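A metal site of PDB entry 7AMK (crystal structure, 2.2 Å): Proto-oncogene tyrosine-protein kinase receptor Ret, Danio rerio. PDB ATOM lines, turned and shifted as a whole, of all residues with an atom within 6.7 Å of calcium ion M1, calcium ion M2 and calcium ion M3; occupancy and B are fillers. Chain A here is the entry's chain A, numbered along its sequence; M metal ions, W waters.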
ATOM      1  N   GLU A 142     -12.522  31.480 -16.490  1.00  0.00           N
ATOM      2  CA  GLU A 142     -13.584  30.589 -16.956  1.00  0.00           C
ATOM      3  C   GLU A 142     -14.006  29.634 -15.827  1.00  0.00           C
ATOM      4  O   GLU A 142     -13.313  29.475 -14.816  1.00  0.00           O
ATOM      5  CB  GLU A 142     -13.081  29.822 -18.197  1.00  0.00           C
ATOM      6  CG  GLU A 142     -11.912  28.912 -17.916  1.00  0.00           C
ATOM      7  CD  GLU A 142     -11.633  27.901 -19.015  1.00  0.00           C
ATOM      8  OE1 GLU A 142     -12.498  27.661 -19.878  1.00  0.00           O
ATOM      9  OE2 GLU A 142     -10.515  27.365 -19.001  1.00  0.00           O
ATOM     10  N   ASN A 143     -15.195  29.036 -15.993  1.00  0.00           N
ATOM     11  CA  ASN A 143     -15.685  27.974 -15.090  1.00  0.00           C
ATOM     12  C   ASN A 143     -15.806  28.435 -13.626  1.00  0.00           C
ATOM     13  O   ASN A 143     -15.484  27.692 -12.705  1.00  0.00           O
ATOM     14  CB  ASN A 143     -14.812  26.719 -15.137  1.00  0.00           C
ATOM     15  CG  ASN A 143     -14.623  26.186 -16.535  1.00  0.00           C
ATOM     16  OD1 ASN A 143     -15.504  26.304 -17.381  1.00  0.00           O
ATOM     17  ND2 ASN A 143     -13.469  25.597 -16.790  1.00  0.00           N
ATOM     18  N   VAL A 193     -18.445  31.025 -17.798  1.00  0.00           N
ATOM     19  CA  VAL A 193     -18.065  31.196 -19.194  1.00  0.00           C
ATOM     20  C   VAL A 193     -16.969  30.172 -19.539  1.00  0.00           C
ATOM     21  O   VAL A 193     -16.456  29.464 -18.674  1.00  0.00           O
ATOM     22  CB  VAL A 193     -17.618  32.644 -19.477  1.00  0.00           C
ATOM     23  CG1 VAL A 193     -18.752  33.563 -19.076  1.00  0.00           C
ATOM     24  CG2 VAL A 193     -16.337  33.010 -18.675  1.00  0.00           C
ATOM     25  N   ASP A 194     -16.659  30.089 -20.830  1.00  0.00           N
ATOM     26  CA  ASP A 194     -15.745  29.075 -21.369  1.00  0.00           C
ATOM     27  C   ASP A 194     -14.696  29.807 -22.184  1.00  0.00           C
ATOM     28  O   ASP A 194     -14.985  30.358 -23.253  1.00  0.00           O
ATOM     29  CB  ASP A 194     -16.519  28.038 -22.201  1.00  0.00           C
ATOM     30  CG  ASP A 194     -15.613  26.934 -22.820  1.00  0.00           C
ATOM     31  OD1 ASP A 194     -14.421  26.843 -22.472  1.00  0.00           O
ATOM     32  OD2 ASP A 194     -16.095  26.174 -23.687  1.00  0.00           O
ATOM     33  N   ARG A 195     -13.465  29.842 -21.659  1.00  0.00           N
ATOM     34  CA  ARG A 195     -12.392  30.527 -22.359  1.00  0.00           C
ATOM     35  C   ARG A 195     -12.256  29.956 -23.776  1.00  0.00           C
ATOM     36  O   ARG A 195     -11.972  30.705 -24.727  1.00  0.00           O
ATOM     37  CB  ARG A 195     -11.084  30.398 -21.574  1.00  0.00           C
ATOM     38  CG  ARG A 195      -9.962  31.350 -22.009  1.00  0.00           C
ATOM     39  CD  ARG A 195      -9.345  31.018 -23.371  1.00  0.00           C
ATOM     40  NE  ARG A 195      -8.795  29.673 -23.413  1.00  0.00           N
ATOM     41  CZ  ARG A 195      -8.063  29.158 -24.396  1.00  0.00           C
ATOM     42  NH1 ARG A 195      -7.720  29.862 -25.465  1.00  0.00           N
ATOM     43  NH2 ARG A 195      -7.665  27.894 -24.310  1.00  0.00           N
ATOM     44  N   GLU A 196     -12.488  28.656 -23.944  1.00  0.00           N
ATOM     45  CA  GLU A 196     -12.351  28.018 -25.252  1.00  0.00           C
ATOM     46  C   GLU A 196     -13.443  28.431 -26.221  1.00  0.00           C
ATOM     47  O   GLU A 196     -13.287  28.260 -27.438  1.00  0.00           O
ATOM     48  CB  GLU A 196     -12.339  26.488 -25.118  1.00  0.00           C
ATOM     49  CG  GLU A 196     -10.952  25.884 -24.788  1.00  0.00           C
ATOM     50  CD  GLU A 196     -10.536  26.038 -23.313  1.00  0.00           C
ATOM     51  OE1 GLU A 196     -11.413  25.968 -22.425  1.00  0.00           O
ATOM     52  OE2 GLU A 196      -9.321  26.214 -23.046  1.00  0.00           O
ATOM     53  N   GLU A 197     -14.558  28.947 -25.745  1.00  0.00           N
ATOM     54  CA  GLU A 197     -15.543  29.486 -26.667  1.00  0.00           C
ATOM     55  C   GLU A 197     -15.250  30.935 -26.990  1.00  0.00           C
ATOM     56  O   GLU A 197     -15.324  31.333 -28.158  1.00  0.00           O
ATOM     57  CB  GLU A 197     -16.960  29.353 -26.102  1.00  0.00           C
ATOM     58  N   TYR A 227      -9.835  34.570 -18.421  1.00  0.00           N
ATOM     59  CA  TYR A 227      -8.639  33.795 -18.115  1.00  0.00           C
ATOM     60  C   TYR A 227      -8.910  32.304 -18.186  1.00  0.00           C
ATOM     61  O   TYR A 227     -10.006  31.827 -17.912  1.00  0.00           O
ATOM     62  CB  TYR A 227      -8.098  34.149 -16.725  1.00  0.00           C
ATOM     63  CG  TYR A 227      -7.444  35.503 -16.664  1.00  0.00           C
ATOM     64  CD1 TYR A 227      -7.359  36.328 -17.784  1.00  0.00           C
ATOM     65  CD2 TYR A 227      -6.889  35.954 -15.481  1.00  0.00           C
ATOM     66  CE1 TYR A 227      -6.738  37.581 -17.718  1.00  0.00           C
ATOM     67  CE2 TYR A 227      -6.270  37.185 -15.398  1.00  0.00           C
ATOM     68  CZ  TYR A 227      -6.204  38.000 -16.510  1.00  0.00           C
ATOM     69  OH  TYR A 227      -5.601  39.223 -16.369  1.00  0.00           O
ATOM     70  N   ASP A 228      -7.871  31.566 -18.541  1.00  0.00           N
ATOM     71  CA  ASP A 228      -7.946  30.154 -18.853  1.00  0.00           C
ATOM     72  C   ASP A 228      -7.634  29.345 -17.615  1.00  0.00           C
ATOM     73  O   ASP A 228      -6.831  29.735 -16.764  1.00  0.00           O
ATOM     74  CB  ASP A 228      -6.949  29.814 -19.958  1.00  0.00           C
ATOM     75  CG  ASP A 228      -7.090  28.421 -20.471  1.00  0.00           C
ATOM     76  OD1 ASP A 228      -8.164  28.109 -20.995  1.00  0.00           O
ATOM     77  OD2 ASP A 228      -6.126  27.644 -20.382  1.00  0.00           O
ATOM     78  N   GLU A 229      -8.258  28.186 -17.516  1.00  0.00           N
ATOM     79  CA  GLU A 229      -7.822  27.191 -16.558  1.00  0.00           C
ATOM     80  C   GLU A 229      -7.613  25.873 -17.287  1.00  0.00           C
ATOM     81  O   GLU A 229      -8.000  25.725 -18.453  1.00  0.00           O
ATOM     82  CB  GLU A 229      -8.815  27.046 -15.402  1.00  0.00           C
ATOM     83  CG  GLU A 229     -10.039  26.283 -15.726  1.00  0.00           C
ATOM     84  CD  GLU A 229     -10.896  26.052 -14.491  1.00  0.00           C
ATOM     85  OE1 GLU A 229     -10.549  26.605 -13.424  1.00  0.00           O
ATOM     86  OE2 GLU A 229     -11.924  25.324 -14.563  1.00  0.00           O
ATOM     87  N   ASP A 230      -6.968  24.928 -16.614  1.00  0.00           N
ATOM     88  CA  ASP A 230      -6.604  23.652 -17.224  1.00  0.00           C
ATOM     89  C   ASP A 230      -7.830  22.749 -17.141  1.00  0.00           C
ATOM     90  O   ASP A 230      -8.068  22.085 -16.135  1.00  0.00           O
ATOM     91  CB  ASP A 230      -5.372  23.063 -16.528  1.00  0.00           C
ATOM     92  CG  ASP A 230      -4.913  21.714 -17.127  1.00  0.00           C
ATOM     93  OD1 ASP A 230      -5.458  21.233 -18.140  1.00  0.00           O
ATOM     94  OD2 ASP A 230      -3.985  21.126 -16.538  1.00  0.00           O
ATOM     95  N   ASP A 231      -8.647  22.760 -18.196  1.00  0.00           N
ATOM     96  CA  ASP A 231      -9.885  21.988 -18.190  1.00  0.00           C
ATOM     97  C   ASP A 231     -10.014  21.155 -19.459  1.00  0.00           C
ATOM     98  O   ASP A 231     -11.133  20.765 -19.823  1.00  0.00           O
ATOM     99  CB  ASP A 231     -11.109  22.909 -17.982  1.00  0.00           C
ATOM    100  CG  ASP A 231     -11.337  23.886 -19.167  1.00  0.00           C
ATOM    101  OD1 ASP A 231     -10.532  23.929 -20.120  1.00  0.00           O
ATOM    102  OD2 ASP A 231     -12.352  24.613 -19.131  1.00  0.00           O
ATOM    103  N   ASN A 232      -8.907  20.882 -20.143  1.00  0.00           N
ATOM    104  CA  ASN A 232      -8.906  20.032 -21.314  1.00  0.00           C
ATOM    105  C   ASN A 232      -7.736  19.067 -21.218  1.00  0.00           C
ATOM    106  O   ASN A 232      -6.618  19.476 -20.921  1.00  0.00           O
ATOM    107  CB  ASN A 232      -8.807  20.857 -22.604  1.00  0.00           C
ATOM    108  CG  ASN A 232     -10.063  21.669 -22.870  1.00  0.00           C
ATOM    109  OD1 ASN A 232     -10.996  21.197 -23.510  1.00  0.00           O
ATOM    110  ND2 ASN A 232     -10.091  22.900 -22.366  1.00  0.00           N
ATOM    111  N   SER A 233      -8.011  17.768 -21.447  1.00  0.00           N
ATOM    112  CA  SER A 233      -6.930  16.819 -21.388  1.00  0.00           C
ATOM    113  C   SER A 233      -6.177  16.753 -22.716  1.00  0.00           C
ATOM    114  O   SER A 233      -6.746  17.028 -23.771  1.00  0.00           O
ATOM    115  CB  SER A 233      -7.449  15.434 -21.048  1.00  0.00           C
ATOM    116  OG  SER A 233      -8.492  15.078 -21.921  1.00  0.00           O
ATOM    117  N   PRO A 234      -4.898  16.402 -22.653  1.00  0.00           N
ATOM    118  CA  PRO A 234      -4.122  16.237 -23.885  1.00  0.00           C
ATOM    119  C   PRO A 234      -4.599  15.033 -24.672  1.00  0.00           C
ATOM    120  O   PRO A 234      -5.193  14.108 -24.147  1.00  0.00           O
ATOM    121  CB  PRO A 234      -2.698  16.043 -23.362  1.00  0.00           C
ATOM    122  CG  PRO A 234      -2.895  15.470 -21.995  1.00  0.00           C
ATOM    123  CD  PRO A 234      -4.089  16.181 -21.453  1.00  0.00           C
ATOM    124  N   ASP A 263      -3.334  20.126 -26.755  1.00  0.00           N
ATOM    125  CA  ASP A 263      -4.094  20.491 -25.566  1.00  0.00           C
ATOM    126  C   ASP A 263      -4.770  21.828 -25.847  1.00  0.00           C
ATOM    127  O   ASP A 263      -4.101  22.801 -26.187  1.00  0.00           O
ATOM    128  CB  ASP A 263      -3.170  20.578 -24.339  1.00  0.00           C
ATOM    129  CG  ASP A 263      -3.923  20.617 -23.022  1.00  0.00           C
ATOM    130  OD1 ASP A 263      -4.880  21.384 -22.894  1.00  0.00           O
ATOM    131  OD2 ASP A 263      -3.544  19.880 -22.098  1.00  0.00           O
ATOM    132  N   ARG A 264      -6.099  21.865 -25.730  1.00  0.00           N
ATOM    133  CA  ARG A 264      -6.828  23.087 -26.063  1.00  0.00           C
ATOM    134  C   ARG A 264      -6.566  24.223 -25.080  1.00  0.00           C
ATOM    135  O   ARG A 264      -6.821  25.389 -25.421  1.00  0.00           O
ATOM    136  CB  ARG A 264      -8.317  22.797 -26.153  1.00  0.00           C
ATOM    137  CG  ARG A 264      -8.625  21.825 -27.277  1.00  0.00           C
ATOM    138  CD  ARG A 264     -10.125  21.669 -27.532  1.00  0.00           C
ATOM    139  NE  ARG A 264     -10.345  20.744 -28.643  1.00  0.00           N
ATOM    140  CZ  ARG A 264     -10.331  21.074 -29.930  1.00  0.00           C
ATOM    141  NH1 ARG A 264     -10.146  22.322 -30.316  1.00  0.00           N
ATOM    142  NH2 ARG A 264     -10.510  20.122 -30.841  1.00  0.00           N
ATOM    143  N   ASP A 265      -6.072  23.918 -23.890  1.00  0.00           N
ATOM    144  CA  ASP A 265      -5.721  24.944 -22.921  1.00  0.00           C
ATOM    145  C   ASP A 265      -4.436  25.680 -23.333  1.00  0.00           C
ATOM    146  O   ASP A 265      -3.571  25.138 -24.024  1.00  0.00           O
ATOM    147  CB  ASP A 265      -5.539  24.329 -21.534  1.00  0.00           C
ATOM    148  CG  ASP A 265      -6.788  23.636 -21.039  1.00  0.00           C
ATOM    149  OD1 ASP A 265      -7.886  24.190 -21.234  1.00  0.00           O
ATOM    150  OD2 ASP A 265      -6.681  22.531 -20.467  1.00  0.00           O
ATOM    151  N   THR A 266      -4.325  26.924 -22.886  1.00  0.00           N
ATOM    152  CA  THR A 266      -3.139  27.743 -23.103  1.00  0.00           C
ATOM    153  C   THR A 266      -2.078  27.450 -22.054  1.00  0.00           C
ATOM    154  O   THR A 266      -2.344  26.904 -20.982  1.00  0.00           O
ATOM    155  CB  THR A 266      -3.486  29.247 -23.049  1.00  0.00           C
ATOM    156  OG1 THR A 266      -3.741  29.625 -21.697  1.00  0.00           O
ATOM    157  CG2 THR A 266      -4.713  29.537 -23.895  1.00  0.00           C
ATOM    158  N   GLN A 276       0.412  25.344 -14.066  1.00  0.00           N
ATOM    159  CA  GLN A 276      -0.855  25.205 -14.772  1.00  0.00           C
ATOM    160  C   GLN A 276      -0.653  24.611 -16.153  1.00  0.00           C
ATOM    161  O   GLN A 276       0.071  25.163 -16.987  1.00  0.00           O
ATOM    162  CB  GLN A 276      -1.554  26.563 -14.893  1.00  0.00           C
ATOM    163  CG  GLN A 276      -2.577  26.626 -16.035  1.00  0.00           C
ATOM    164  CD  GLN A 276      -3.523  27.826 -15.963  1.00  0.00           C
ATOM    165  OE1 GLN A 276      -3.544  28.584 -14.980  1.00  0.00           O
ATOM    166  NE2 GLN A 276      -4.335  27.999 -17.006  1.00  0.00           N
ATOM    167  N   ASN A 277      -1.312  23.486 -16.406  1.00  0.00           N
ATOM    168  CA  ASN A 277      -1.328  22.890 -17.737  1.00  0.00           C
ATOM    169  C   ASN A 277       0.018  22.328 -18.140  1.00  0.00           C
ATOM    170  O   ASN A 277       0.234  22.036 -19.307  1.00  0.00           O
ATOM    171  CB  ASN A 277      -1.785  23.879 -18.811  1.00  0.00           C
ATOM    172  CG  ASN A 277      -2.505  23.195 -19.921  1.00  0.00           C
ATOM    173  OD1 ASN A 277      -3.297  22.298 -19.672  1.00  0.00           O
ATOM    174  ND2 ASN A 277      -2.210  23.563 -21.159  1.00  0.00           N
ATOM    175  N   LEU A 279       2.542  19.547 -18.799  1.00  0.00           N
ATOM    176  CA  LEU A 279       2.604  18.112 -19.019  1.00  0.00           C
ATOM    177  C   LEU A 279       3.988  17.593 -18.616  1.00  0.00           C
ATOM    178  O   LEU A 279       4.997  18.065 -19.124  1.00  0.00           O
ATOM    179  CB  LEU A 279       2.341  17.748 -20.488  1.00  0.00           C
ATOM    180  CG  LEU A 279       1.064  18.273 -21.157  1.00  0.00           C
ATOM    181  CD1 LEU A 279       0.980  17.758 -22.613  1.00  0.00           C
ATOM    182  CD2 LEU A 279      -0.113  17.835 -20.329  1.00  0.00           C
ATOM    183  N   ASP A 341      -0.955  15.395 -17.849  1.00  0.00           N
ATOM    184  CA  ASP A 341      -1.423  16.760 -17.575  1.00  0.00           C
ATOM    185  C   ASP A 341      -1.700  16.875 -16.078  1.00  0.00           C
ATOM    186  O   ASP A 341      -2.772  16.487 -15.609  1.00  0.00           O
ATOM    187  CB  ASP A 341      -2.663  17.076 -18.390  1.00  0.00           C
ATOM    188  CG  ASP A 341      -3.130  18.545 -18.224  1.00  0.00           C
ATOM    189  OD1 ASP A 341      -2.666  19.274 -17.296  1.00  0.00           O
ATOM    190  OD2 ASP A 341      -3.964  18.959 -19.068  1.00  0.00           O
ATOM    191  N   THR A 343      -2.270  19.183 -13.658  1.00  0.00           N
ATOM    192  CA  THR A 343      -3.348  19.960 -13.075  1.00  0.00           C
ATOM    193  C   THR A 343      -4.699  19.713 -13.735  1.00  0.00           C
ATOM    194  O   THR A 343      -5.643  20.469 -13.483  1.00  0.00           O
ATOM    195  CB  THR A 343      -3.020  21.471 -13.132  1.00  0.00           C
ATOM    196  OG1 THR A 343      -2.677  21.831 -14.465  1.00  0.00           O
ATOM    197  CG2 THR A 343      -1.839  21.797 -12.245  1.00  0.00           C
ATOM    198  N   PHE A 344      -4.813  18.714 -14.606  1.00  0.00           N
ATOM    199  CA  PHE A 344      -6.130  18.388 -15.144  1.00  0.00           C
ATOM    200  C   PHE A 344      -6.915  17.569 -14.118  1.00  0.00           C
ATOM    201  O   PHE A 344      -6.452  16.502 -13.705  1.00  0.00           O
ATOM    202  CB  PHE A 344      -6.032  17.640 -16.459  1.00  0.00           C
ATOM    203  CG  PHE A 344      -7.372  17.265 -17.028  1.00  0.00           C
ATOM    204  CD1 PHE A 344      -8.138  18.188 -17.720  1.00  0.00           C
ATOM    205  CD2 PHE A 344      -7.880  15.985 -16.839  1.00  0.00           C
ATOM    206  CE1 PHE A 344      -9.389  17.850 -18.231  1.00  0.00           C
ATOM    207  CE2 PHE A 344      -9.118  15.636 -17.361  1.00  0.00           C
ATOM    208  CZ  PHE A 344      -9.874  16.564 -18.046  1.00  0.00           C
HETATM  209 CA    CA M   1     -13.136  25.742 -20.929  1.00  0.00          CA
HETATM  210 CA    CA M   2      -9.259  25.994 -20.487  1.00  0.00          CA
HETATM  211 CA    CA M   3      -4.930  20.889 -20.388  1.00  0.00          CA
HETATM  212  O   HOH W   1     -13.612  23.731 -22.019  1.00  0.00           O
HETATM  213  O   HOH W   2     -15.079  25.810 -19.650  1.00  0.00           O
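ND2 of Asn 232 lies close to OD1 of Asp 231, 2.5 Å away.
ND2 of Asn 143 sits close to OD2 of Asp 231, 2.8 Å away.
ND2 of Asn 232 sits close to OE1 of Glu 196 (3.3 Å).
The backbone NH (N) of Glu 142 sits at hydrogen-bond distance from the backbone carbonyl oxygen (O) of Tyr 227.
The backbone NH of Phe 344 sits at hydrogen-bond distance from the side-chain carboxylate of Asp 230 (3.2 Å).
ND2 of Asn 143 is in hydrogen-bond range of OE2 of Glu 229 (2.7 Å).
O of Asp 228 lies within hydrogen-bond range of NE2 of Gln 276.
N of Phe 344 is in hydrogen-bond range of OD1 of Asp 341 (3.5 Å).
Of the 25 residues printed, 4 come within 4 Å of calcium ion M1.
The nearest printed residue that does not touch calcium ion M1 is Asn 143 (4.2 Å).
Within 4 Å of calcium ion M2: Glu 142, Glu 196, Asp 228, Glu 229, Asp 231, Asn 232 and Asp 265.
Along chain A the residues within 4 Å of calcium ion M2 span positions 142 to 265.
The nearest printed residue that does not touch calcium ion M2 is Arg 195 (4.6 Å).
Within 4 Å of calcium ion M3: Asp 230, Asn 232, Asp 263, Asp 265, Asn 277 and Asp 341.
Calcium ion M1 is bound by the side-chain carboxylate of Asp 231 (2.3 Å), the side-chain carboxylate of Glu 142 (2.3 Å), the side-chain carboxylate of Asp 194 (2.3 Å), the side-chain carboxylate of Glu 196 (2.3 Å), water W2 (2.3 Å) and water W1 (2.3 Å).
Calcium ion M1 has six donor atoms within binding distance.
OE2 of Glu 142 is bound to calcium ion M2, at 2.4 Å.
Calcium ion M2 is bound by OD1 of Asp 265 (2.4 Å).
O of Glu 229 binds calcium ion M2, at 2.4 Å.
Calcium ion M2 is bound by OD1 of Asp 228.
Calcium ion M2 is bound by the side-chain carboxylate (OD1) of Asp 231 (2.5 Å).
OE2 of Glu 196 binds calcium ion M2, at 2.6 Å.
OE1 of Glu 196 is bound to calcium ion M2 (2.9 Å).
Calcium ion M2 has seven donor atoms within binding distance.
Calcium ion M3 is bound by O of Asn 232 (2.3 Å), OD1 of Asn 277 (2.3 Å), OD1 of Asp 230 (2.3 Å), OD2 of Asp 265 (2.4 Å), OD2 of Asp 263 (2.4 Å), OD2 of Asp 341 (2.5 Å) and OD1 of Asp 263 (2.6 Å).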
